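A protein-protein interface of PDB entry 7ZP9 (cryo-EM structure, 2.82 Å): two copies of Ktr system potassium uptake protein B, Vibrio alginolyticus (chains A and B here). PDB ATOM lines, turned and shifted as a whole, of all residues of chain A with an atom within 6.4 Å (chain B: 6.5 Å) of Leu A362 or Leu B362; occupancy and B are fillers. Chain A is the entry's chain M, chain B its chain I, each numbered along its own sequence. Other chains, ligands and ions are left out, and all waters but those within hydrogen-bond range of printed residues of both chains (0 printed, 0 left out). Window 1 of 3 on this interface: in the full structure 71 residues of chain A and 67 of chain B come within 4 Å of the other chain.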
ATOM      1  N   THR A 328      -2.859   6.359  18.988  1.00  0.00           N
ATOM      2  CA  THR A 328      -1.787   6.036  19.925  1.00  0.00           C
ATOM      3  C   THR A 328      -0.670   7.067  19.852  1.00  0.00           C
ATOM      4  O   THR A 328      -0.167   7.531  20.880  1.00  0.00           O
ATOM      5  CB  THR A 328      -1.240   4.641  19.635  1.00  0.00           C
ATOM      6  OG1 THR A 328      -2.312   3.691  19.637  1.00  0.00           O
ATOM      7  CG2 THR A 328      -0.209   4.244  20.672  1.00  0.00           C
ATOM      8  N   VAL A 331      -2.007  10.470  21.358  1.00  0.00           N
ATOM      9  CA  VAL A 331      -2.026  10.505  22.818  1.00  0.00           C
ATOM     10  C   VAL A 331      -0.613  10.651  23.365  1.00  0.00           C
ATOM     11  O   VAL A 331      -0.362  11.461  24.264  1.00  0.00           O
ATOM     12  CB  VAL A 331      -2.723   9.254  23.382  1.00  0.00           C
ATOM     13  CG1 VAL A 331      -2.655   9.254  24.898  1.00  0.00           C
ATOM     14  CG2 VAL A 331      -4.165   9.210  22.932  1.00  0.00           C
ATOM     15  N   ALA A 332       0.332   9.882  22.826  1.00  0.00           N
ATOM     16  CA  ALA A 332       1.719   9.992  23.268  1.00  0.00           C
ATOM     17  C   ALA A 332       2.302  11.353  22.913  1.00  0.00           C
ATOM     18  O   ALA A 332       3.100  11.915  23.669  1.00  0.00           O
ATOM     19  CB  ALA A 332       2.554   8.871  22.653  1.00  0.00           C
ATOM     20  N   ALA A 335       0.632  13.634  25.431  1.00  0.00           N
ATOM     21  CA  ALA A 335       1.139  13.305  26.759  1.00  0.00           C
ATOM     22  C   ALA A 335       2.535  13.876  26.955  1.00  0.00           C
ATOM     23  O   ALA A 335       2.850  14.418  28.019  1.00  0.00           O
ATOM     24  CB  ALA A 335       1.143  11.794  26.974  1.00  0.00           C
ATOM     25  N   THR A 336       3.382  13.772  25.928  1.00  0.00           N
ATOM     26  CA  THR A 336       4.707  14.378  25.981  1.00  0.00           C
ATOM     27  C   THR A 336       4.608  15.888  26.143  1.00  0.00           C
ATOM     28  O   THR A 336       5.320  16.487  26.957  1.00  0.00           O
ATOM     29  CB  THR A 336       5.489  14.025  24.715  1.00  0.00           C
ATOM     30  OG1 THR A 336       5.853  12.640  24.745  1.00  0.00           O
ATOM     31  CG2 THR A 336       6.739  14.881  24.592  1.00  0.00           C
ATOM     32  N   PHE A 339       3.646  16.593  29.639  1.00  0.00           N
ATOM     33  CA  PHE A 339       4.728  16.364  30.592  1.00  0.00           C
ATOM     34  C   PHE A 339       5.759  17.484  30.550  1.00  0.00           C
ATOM     35  O   PHE A 339       6.258  17.915  31.595  1.00  0.00           O
ATOM     36  CB  PHE A 339       5.399  15.018  30.318  1.00  0.00           C
ATOM     37  CG  PHE A 339       4.486  13.839  30.477  1.00  0.00           C
ATOM     38  CD1 PHE A 339       3.370  13.914  31.288  1.00  0.00           C
ATOM     39  CD2 PHE A 339       4.746  12.652  29.813  1.00  0.00           C
ATOM     40  CE1 PHE A 339       2.530  12.829  31.434  1.00  0.00           C
ATOM     41  CE2 PHE A 339       3.908  11.566  29.955  1.00  0.00           C
ATOM     42  CZ  PHE A 339       2.799  11.654  30.768  1.00  0.00           C
ATOM     43  N   THR A 357      -5.063   5.160  29.701  1.00  0.00           N
ATOM     44  CA  THR A 357      -4.924   5.338  28.258  1.00  0.00           C
ATOM     45  C   THR A 357      -3.532   5.832  27.892  1.00  0.00           C
ATOM     46  O   THR A 357      -2.946   5.386  26.901  1.00  0.00           O
ATOM     47  CB  THR A 357      -5.985   6.308  27.736  1.00  0.00           C
ATOM     48  OG1 THR A 357      -7.271   5.931  28.240  1.00  0.00           O
ATOM     49  CG2 THR A 357      -6.018   6.295  26.218  1.00  0.00           C
ATOM     50  N   VAL A 358      -2.990   6.766  28.677  1.00  0.00           N
ATOM     51  CA  VAL A 358      -1.642   7.266  28.425  1.00  0.00           C
ATOM     52  C   VAL A 358      -0.623   6.148  28.582  1.00  0.00           C
ATOM     53  O   VAL A 358       0.307   6.017  27.778  1.00  0.00           O
ATOM     54  CB  VAL A 358      -1.332   8.449  29.357  1.00  0.00           C
ATOM     55  CG1 VAL A 358       0.050   9.007  29.071  1.00  0.00           C
ATOM     56  CG2 VAL A 358      -2.385   9.524  29.201  1.00  0.00           C
ATOM     57  N   THR A 359      -0.779   5.327  29.622  1.00  0.00           N
ATOM     58  CA  THR A 359       0.122   4.200  29.820  1.00  0.00           C
ATOM     59  C   THR A 359       0.016   3.200  28.676  1.00  0.00           C
ATOM     60  O   THR A 359       1.022   2.612  28.265  1.00  0.00           O
ATOM     61  CB  THR A 359      -0.173   3.524  31.158  1.00  0.00           C
ATOM     62  OG1 THR A 359      -0.164   4.508  32.199  1.00  0.00           O
ATOM     63  CG2 THR A 359       0.872   2.465  31.467  1.00  0.00           C
ATOM     64  N   LYS A 360      -1.193   2.993  28.149  1.00  0.00           N
ATOM     65  CA  LYS A 360      -1.360   2.101  27.006  1.00  0.00           C
ATOM     66  C   LYS A 360      -0.583   2.603  25.798  1.00  0.00           C
ATOM     67  O   LYS A 360       0.124   1.837  25.136  1.00  0.00           O
ATOM     68  CB  LYS A 360      -2.842   1.956  26.655  1.00  0.00           C
ATOM     69  CG  LYS A 360      -3.621   1.030  27.563  1.00  0.00           C
ATOM     70  CD  LYS A 360      -5.044   0.855  27.069  1.00  0.00           C
ATOM     71  CE  LYS A 360      -5.944   0.329  28.171  1.00  0.00           C
ATOM     72  NZ  LYS A 360      -7.381   0.405  27.792  1.00  0.00           N
ATOM     73  N   SER A 361      -0.703   3.897  25.495  1.00  0.00           N
ATOM     74  CA  SER A 361      -0.037   4.446  24.319  1.00  0.00           C
ATOM     75  C   SER A 361       1.477   4.383  24.462  1.00  0.00           C
ATOM     76  O   SER A 361       2.184   4.002  23.524  1.00  0.00           O
ATOM     77  CB  SER A 361      -0.501   5.882  24.079  1.00  0.00           C
ATOM     78  OG  SER A 361       0.309   6.802  24.786  1.00  0.00           O
ATOM     79  N   LEU A 362       1.996   4.754  25.634  1.00  0.00           N
ATOM     80  CA  LEU A 362       3.438   4.708  25.846  1.00  0.00           C
ATOM     81  C   LEU A 362       3.955   3.276  25.846  1.00  0.00           C
ATOM     82  O   LEU A 362       5.038   3.003  25.318  1.00  0.00           O
ATOM     83  CB  LEU A 362       3.803   5.409  27.154  1.00  0.00           C
ATOM     84  CG  LEU A 362       3.424   6.884  27.281  1.00  0.00           C
ATOM     85  CD1 LEU A 362       3.764   7.400  28.668  1.00  0.00           C
ATOM     86  CD2 LEU A 362       4.113   7.712  26.217  1.00  0.00           C
ATOM     87  N   ALA A 363       3.200   2.346  26.438  1.00  0.00           N
ATOM     88  CA  ALA A 363       3.637   0.955  26.476  1.00  0.00           C
ATOM     89  C   ALA A 363       3.704   0.354  25.080  1.00  0.00           C
ATOM     90  O   ALA A 363       4.622  -0.412  24.772  1.00  0.00           O
ATOM     91  CB  ALA A 363       2.706   0.131  27.364  1.00  0.00           C
ATOM     92  N   ILE A 364       2.737   0.686  24.222  1.00  0.00           N
ATOM     93  CA  ILE A 364       2.732   0.152  22.864  1.00  0.00           C
ATOM     94  C   ILE A 364       3.979   0.592  22.110  1.00  0.00           C
ATOM     95  O   ILE A 364       4.626  -0.213  21.430  1.00  0.00           O
ATOM     96  CB  ILE A 364       1.444   0.569  22.129  1.00  0.00           C
ATOM     97  CG1 ILE A 364       0.250  -0.232  22.654  1.00  0.00           C
ATOM     98  CG2 ILE A 364       1.596   0.390  20.628  1.00  0.00           C
ATOM     99  CD1 ILE A 364      -1.080   0.451  22.449  1.00  0.00           C
ATOM    100  N   ILE A 365       4.342   1.870  22.223  1.00  0.00           N
ATOM    101  CA  ILE A 365       5.526   2.372  21.531  1.00  0.00           C
ATOM    102  C   ILE A 365       6.787   1.713  22.075  1.00  0.00           C
ATOM    103  O   ILE A 365       7.684   1.328  21.317  1.00  0.00           O
ATOM    104  CB  ILE A 365       5.599   3.905  21.634  1.00  0.00           C
ATOM    105  CG1 ILE A 365       4.288   4.528  21.159  1.00  0.00           C
ATOM    106  CG2 ILE A 365       6.770   4.441  20.834  1.00  0.00           C
ATOM    107  CD1 ILE A 365       4.216   6.010  21.371  1.00  0.00           C
ATOM    108  N   VAL A 366       6.880   1.583  23.399  1.00  0.00           N
ATOM    109  CA  VAL A 366       8.069   0.989  24.001  1.00  0.00           C
ATOM    110  C   VAL A 366       8.169  -0.492  23.651  1.00  0.00           C
ATOM    111  O   VAL A 366       9.243  -0.985  23.289  1.00  0.00           O
ATOM    112  CB  VAL A 366       8.069   1.218  25.522  1.00  0.00           C
ATOM    113  CG1 VAL A 366       9.134   0.368  26.187  1.00  0.00           C
ATOM    114  CG2 VAL A 366       8.288   2.688  25.828  1.00  0.00           C
ATOM    115  N   VAL A 367       7.059  -1.224  23.754  1.00  0.00           N
ATOM    116  CA  VAL A 367       7.078  -2.642  23.411  1.00  0.00           C
ATOM    117  C   VAL A 367       7.359  -2.833  21.926  1.00  0.00           C
ATOM    118  O   VAL A 367       8.126  -3.719  21.538  1.00  0.00           O
ATOM    119  CB  VAL A 367       5.763  -3.318  23.836  1.00  0.00           C
ATOM    120  CG1 VAL A 367       5.700  -4.736  23.303  1.00  0.00           C
ATOM    121  CG2 VAL A 367       5.645  -3.328  25.348  1.00  0.00           C
ATOM    122  N   THR B 328      15.596   2.923  34.892  1.00  0.00           N
ATOM    123  CA  THR B 328      14.504   3.193  33.961  1.00  0.00           C
ATOM    124  C   THR B 328      14.304   2.029  32.998  1.00  0.00           C
ATOM    125  O   THR B 328      13.173   1.586  32.764  1.00  0.00           O
ATOM    126  CB  THR B 328      14.783   4.480  33.188  1.00  0.00           C
ATOM    127  OG1 THR B 328      15.068   5.541  34.106  1.00  0.00           O
ATOM    128  CG2 THR B 328      13.595   4.858  32.329  1.00  0.00           C
ATOM    129  N   VAL B 331      12.644  -0.952  34.860  1.00  0.00           N
ATOM    130  CA  VAL B 331      11.187  -0.798  35.143  1.00  0.00           C
ATOM    131  C   VAL B 331      10.403  -1.020  33.847  1.00  0.00           C
ATOM    132  O   VAL B 331       9.391  -1.716  33.898  1.00  0.00           O
ATOM    133  CB  VAL B 331      10.871   0.562  35.792  1.00  0.00           C
ATOM    134  CG1 VAL B 331       9.377   0.757  35.988  1.00  0.00           C
ATOM    135  CG2 VAL B 331      11.613   0.746  37.104  1.00  0.00           C
ATOM    136  N   ALA B 332      10.874  -0.482  32.727  1.00  0.00           N
ATOM    137  CA  ALA B 332      10.206  -0.664  31.418  1.00  0.00           C
ATOM    138  C   ALA B 332      10.275  -2.127  30.980  1.00  0.00           C
ATOM    139  O   ALA B 332       9.272  -2.625  30.470  1.00  0.00           O
ATOM    140  CB  ALA B 332      10.841   0.246  30.404  1.00  0.00           C
ATOM    141  N   ALA B 335       7.899  -3.887  33.337  1.00  0.00           N
ATOM    142  CA  ALA B 335       6.511  -3.489  33.016  1.00  0.00           C
ATOM    143  C   ALA B 335       6.067  -4.232  31.759  1.00  0.00           C
ATOM    144  O   ALA B 335       4.935  -4.717  31.743  1.00  0.00           O
ATOM    145  CB  ALA B 335       6.431  -2.005  32.821  1.00  0.00           C
ATOM    146  N   THR B 336       6.942  -4.330  30.761  1.00  0.00           N
ATOM    147  CA  THR B 336       6.617  -5.041  29.502  1.00  0.00           C
ATOM    148  C   THR B 336       6.250  -6.483  29.822  1.00  0.00           C
ATOM    149  O   THR B 336       5.227  -6.945  29.315  1.00  0.00           O
ATOM    150  CB  THR B 336       7.803  -5.019  28.537  1.00  0.00           C
ATOM    151  OG1 THR B 336       7.984  -3.670  28.109  1.00  0.00           O
ATOM    152  CG2 THR B 336       7.606  -5.918  27.337  1.00  0.00           C
ATOM    153  N   PHE B 339       2.869  -6.664  31.373  1.00  0.00           N
ATOM    154  CA  PHE B 339       1.777  -6.409  30.398  1.00  0.00           C
ATOM    155  C   PHE B 339       1.590  -7.619  29.484  1.00  0.00           C
ATOM    156  O   PHE B 339       0.448  -7.941  29.156  1.00  0.00           O
ATOM    157  CB  PHE B 339       2.091  -5.163  29.572  1.00  0.00           C
ATOM    158  CG  PHE B 339       2.289  -3.891  30.352  1.00  0.00           C
ATOM    159  CD1 PHE B 339       1.644  -3.686  31.559  1.00  0.00           C
ATOM    160  CD2 PHE B 339       3.108  -2.885  29.866  1.00  0.00           C
ATOM    161  CE1 PHE B 339       1.823  -2.509  32.268  1.00  0.00           C
ATOM    162  CE2 PHE B 339       3.286  -1.708  30.575  1.00  0.00           C
ATOM    163  CZ  PHE B 339       2.642  -1.523  31.774  1.00  0.00           C
ATOM    164  N   THR B 357       5.583   5.529  38.555  1.00  0.00           N
ATOM    165  CA  THR B 357       6.959   5.191  38.192  1.00  0.00           C
ATOM    166  C   THR B 357       7.036   4.560  36.805  1.00  0.00           C
ATOM    167  O   THR B 357       7.922   4.894  36.007  1.00  0.00           O
ATOM    168  CB  THR B 357       7.565   4.251  39.235  1.00  0.00           C
ATOM    169  OG1 THR B 357       7.286   4.747  40.548  1.00  0.00           O
ATOM    170  CG2 THR B 357       9.066   4.143  39.049  1.00  0.00           C
ATOM    171  N   VAL B 358       6.118   3.640  36.505  1.00  0.00           N
ATOM    172  CA  VAL B 358       6.087   3.013  35.187  1.00  0.00           C
ATOM    173  C   VAL B 358       5.819   4.056  34.113  1.00  0.00           C
ATOM    174  O   VAL B 358       6.442   4.048  33.043  1.00  0.00           O
ATOM    175  CB  VAL B 358       5.036   1.887  35.162  1.00  0.00           C
ATOM    176  CG1 VAL B 358       4.971   1.247  33.787  1.00  0.00           C
ATOM    177  CG2 VAL B 358       5.349   0.850  36.224  1.00  0.00           C
ATOM    178  N   THR B 359       4.882   4.967  34.382  1.00  0.00           N
ATOM    179  CA  THR B 359       4.592   6.040  33.441  1.00  0.00           C
ATOM    180  C   THR B 359       5.805   6.938  33.241  1.00  0.00           C
ATOM    181  O   THR B 359       6.089   7.357  32.116  1.00  0.00           O
ATOM    182  CB  THR B 359       3.392   6.852  33.923  1.00  0.00           C
ATOM    183  OG1 THR B 359       2.283   5.973  34.148  1.00  0.00           O
ATOM    184  CG2 THR B 359       2.999   7.892  32.889  1.00  0.00           C
ATOM    185  N   LYS B 360       6.536   7.239  34.317  1.00  0.00           N
ATOM    186  CA  LYS B 360       7.754   8.035  34.191  1.00  0.00           C
ATOM    187  C   LYS B 360       8.764   7.347  33.287  1.00  0.00           C
ATOM    188  O   LYS B 360       9.344   7.977  32.397  1.00  0.00           O
ATOM    189  CB  LYS B 360       8.374   8.287  35.565  1.00  0.00           C
ATOM    190  CG  LYS B 360       7.702   9.362  36.391  1.00  0.00           C
ATOM    191  CD  LYS B 360       8.541   9.694  37.613  1.00  0.00           C
ATOM    192  CE  LYS B 360       7.725  10.412  38.673  1.00  0.00           C
ATOM    193  NZ  LYS B 360       6.563   9.601  39.124  1.00  0.00           N
ATOM    194  N   SER B 361       8.990   6.051  33.502  1.00  0.00           N
ATOM    195  CA  SER B 361       9.982   5.336  32.701  1.00  0.00           C
ATOM    196  C   SER B 361       9.581   5.300  31.229  1.00  0.00           C
ATOM    197  O   SER B 361      10.391   5.601  30.340  1.00  0.00           O
ATOM    198  CB  SER B 361      10.173   3.923  33.249  1.00  0.00           C
ATOM    199  OG  SER B 361       9.195   3.041  32.733  1.00  0.00           O
ATOM    200  N   LEU B 362       8.323   4.944  30.954  1.00  0.00           N
ATOM    201  CA  LEU B 362       7.864   4.883  29.571  1.00  0.00           C
ATOM    202  C   LEU B 362       7.909   6.256  28.911  1.00  0.00           C
ATOM    203  O   LEU B 362       8.307   6.376  27.747  1.00  0.00           O
ATOM    204  CB  LEU B 362       6.454   4.300  29.508  1.00  0.00           C
ATOM    205  CG  LEU B 362       6.266   2.884  30.054  1.00  0.00           C
ATOM    206  CD1 LEU B 362       4.813   2.456  29.939  1.00  0.00           C
ATOM    207  CD2 LEU B 362       7.173   1.904  29.337  1.00  0.00           C
ATOM    208  N   ALA B 363       7.509   7.303  29.637  1.00  0.00           N
ATOM    209  CA  ALA B 363       7.542   8.650  29.084  1.00  0.00           C
ATOM    210  C   ALA B 363       8.966   9.092  28.797  1.00  0.00           C
ATOM    211  O   ALA B 363       9.223   9.747  27.783  1.00  0.00           O
ATOM    212  CB  ALA B 363       6.863   9.626  30.042  1.00  0.00           C
ATOM    213  N   ILE B 364       9.906   8.750  29.680  1.00  0.00           N
ATOM    214  CA  ILE B 364      11.304   9.083  29.431  1.00  0.00           C
ATOM    215  C   ILE B 364      11.784   8.418  28.153  1.00  0.00           C
ATOM    216  O   ILE B 364      12.416   9.059  27.305  1.00  0.00           O
ATOM    217  CB  ILE B 364      12.177   8.694  30.639  1.00  0.00           C
ATOM    218  CG1 ILE B 364      11.958   9.670  31.796  1.00  0.00           C
ATOM    219  CG2 ILE B 364      13.643   8.639  30.249  1.00  0.00           C
ATOM    220  CD1 ILE B 364      12.288   9.093  33.151  1.00  0.00           C
ATOM    221  N   ILE B 365      11.464   7.134  27.974  1.00  0.00           N
ATOM    222  CA  ILE B 365      11.905   6.438  26.765  1.00  0.00           C
ATOM    223  C   ILE B 365      11.286   7.064  25.519  1.00  0.00           C
ATOM    224  O   ILE B 365      11.970   7.287  24.513  1.00  0.00           O
ATOM    225  CB  ILE B 365      11.597   4.934  26.858  1.00  0.00           C
ATOM    226  CG1 ILE B 365      12.236   4.345  28.112  1.00  0.00           C
ATOM    227  CG2 ILE B 365      12.085   4.212  25.618  1.00  0.00           C
ATOM    228  CD1 ILE B 365      11.871   2.918  28.345  1.00  0.00           C
ATOM    229  N   VAL B 366       9.986   7.365  25.564  1.00  0.00           N
ATOM    230  CA  VAL B 366       9.309   7.892  24.379  1.00  0.00           C
ATOM    231  C   VAL B 366       9.823   9.286  24.030  1.00  0.00           C
ATOM    232  O   VAL B 366      10.080   9.593  22.859  1.00  0.00           O
ATOM    233  CB  VAL B 366       7.784   7.881  24.579  1.00  0.00           C
ATOM    234  CG1 VAL B 366       7.093   8.483  23.373  1.00  0.00           C
ATOM    235  CG2 VAL B 366       7.300   6.460  24.786  1.00  0.00           C
ATOM    236  N   VAL B 367       9.974  10.154  25.032  1.00  0.00           N
ATOM    237  CA  VAL B 367      10.470  11.502  24.773  1.00  0.00           C
ATOM    238  C   VAL B 367      11.908  11.456  24.273  1.00  0.00           C
ATOM    239  O   VAL B 367      12.287  12.204  23.361  1.00  0.00           O
ATOM    240  CB  VAL B 367      10.328  12.373  26.033  1.00  0.00           C
ATOM    241  CG1 VAL B 367      10.963  13.729  25.816  1.00  0.00           C
ATOM    242  CG2 VAL B 367       8.865  12.535  26.395  1.00  0.00           C
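OG1 of Thr A359 lies within hydrogen-bond range of OG1 of Thr B359 (3.5 Å).
The side-chain hydroxyl of Thr B336 is in hydrogen-bond range of the backbone carbonyl oxygen of Ala B332, at 2.9 Å.
The backbone carbonyl oxygen of Ala A332 is in hydrogen-bond range of the side-chain hydroxyl of Thr A336 (3.0 Å).
CG2 of Val B367 touches OG1 of Thr A336, 3.4 Å away.
CE2 of Phe A339 touches CB of Ala B363, at 3.5 Å.
Leu A362 touches Leu B362 (CB to CB, 3.7 Å).
Ala B363 touches Leu A362.
Val B366 touches Leu A362 (CG2 to CD2, 3.7 Å).
Ala A363 touches Phe B339.
Ala A363 touches Leu B362 (N to CD1, 3.9 Å).
CD2 of Leu B362 touches CG2 of Val A366 (3.8 Å).
Val A367 touches Thr B336 (CG2 to OG1, 3.6 Å).
Of the printed residues of chain B, Leu A362 touches Leu B362 (3.7 Å), Ala B363 (3.9 Å) and Val B366 (3.7 Å).
Of the printed residues of chain A, Thr B359 touches Thr A359 (3.5 Å).
Printed residues of chain A within 4 Å of Ala B363: Phe A339 (3.5 Å) and Leu A362 (3.9 Å).
Of the printed residues of chain B, Thr A359 touches Thr B359 (3.5 Å).
Printed residues of chain B within 4 Å of Thr A336: Val B367.
Val B358 touches none of the printed residues of chain A.
The nearest printed residue of chain A that does not touch Val B367 is Phe A339 (5.4 Å).
Of the 17 printed residues of chain A, 7 touch a printed residue of chain B.
Printed residues of chain A that touch a printed residue of chain B: Thr A336, Phe A339, Thr A359, Leu A362, Ala A363, Val A366 and Val A367.
Hydrophobic or aromatic side chains of chain A within 4 Å of the printed part of chain B: Phe A339, Leu A362, Ala A363, Val A366 and Val A367.
Of the 17 printed residues of chain B, 7 touch a printed residue of chain A.
Hydrophobic or aromatic side chains of chain B that line the printed part of chain A: Phe B339, Leu B362, Ala B363, Val B366 and Val B367.
Along chain B the printed residues that touch a printed residue of chain A span positions 336 to 367.
Among the printed residues, no Asp or Glu carboxylate lies within 4 Å of a Lys or Arg side-chain nitrogen of the other chain.
Phe A339 touches Ala B363, and with the chains exchanged Ala A363 touches Phe B339.
Thr B359 touches its own counterpart, Thr A359.
Leu A362 touches its own counterpart, Leu B362.
Leu A362 touches Ala B363, and with the chains exchanged Ala A363 touches Leu B362.
Positions printed for both chains: 328, 331, 332, 335, 336, 339, 357, 358, 359, 360, 361, 362, 363, 364, 365, 366 and 367.
Of the 10 pairs that touch across the chains among the printed residues, 10 have their exchanged pair printed and touching as well.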
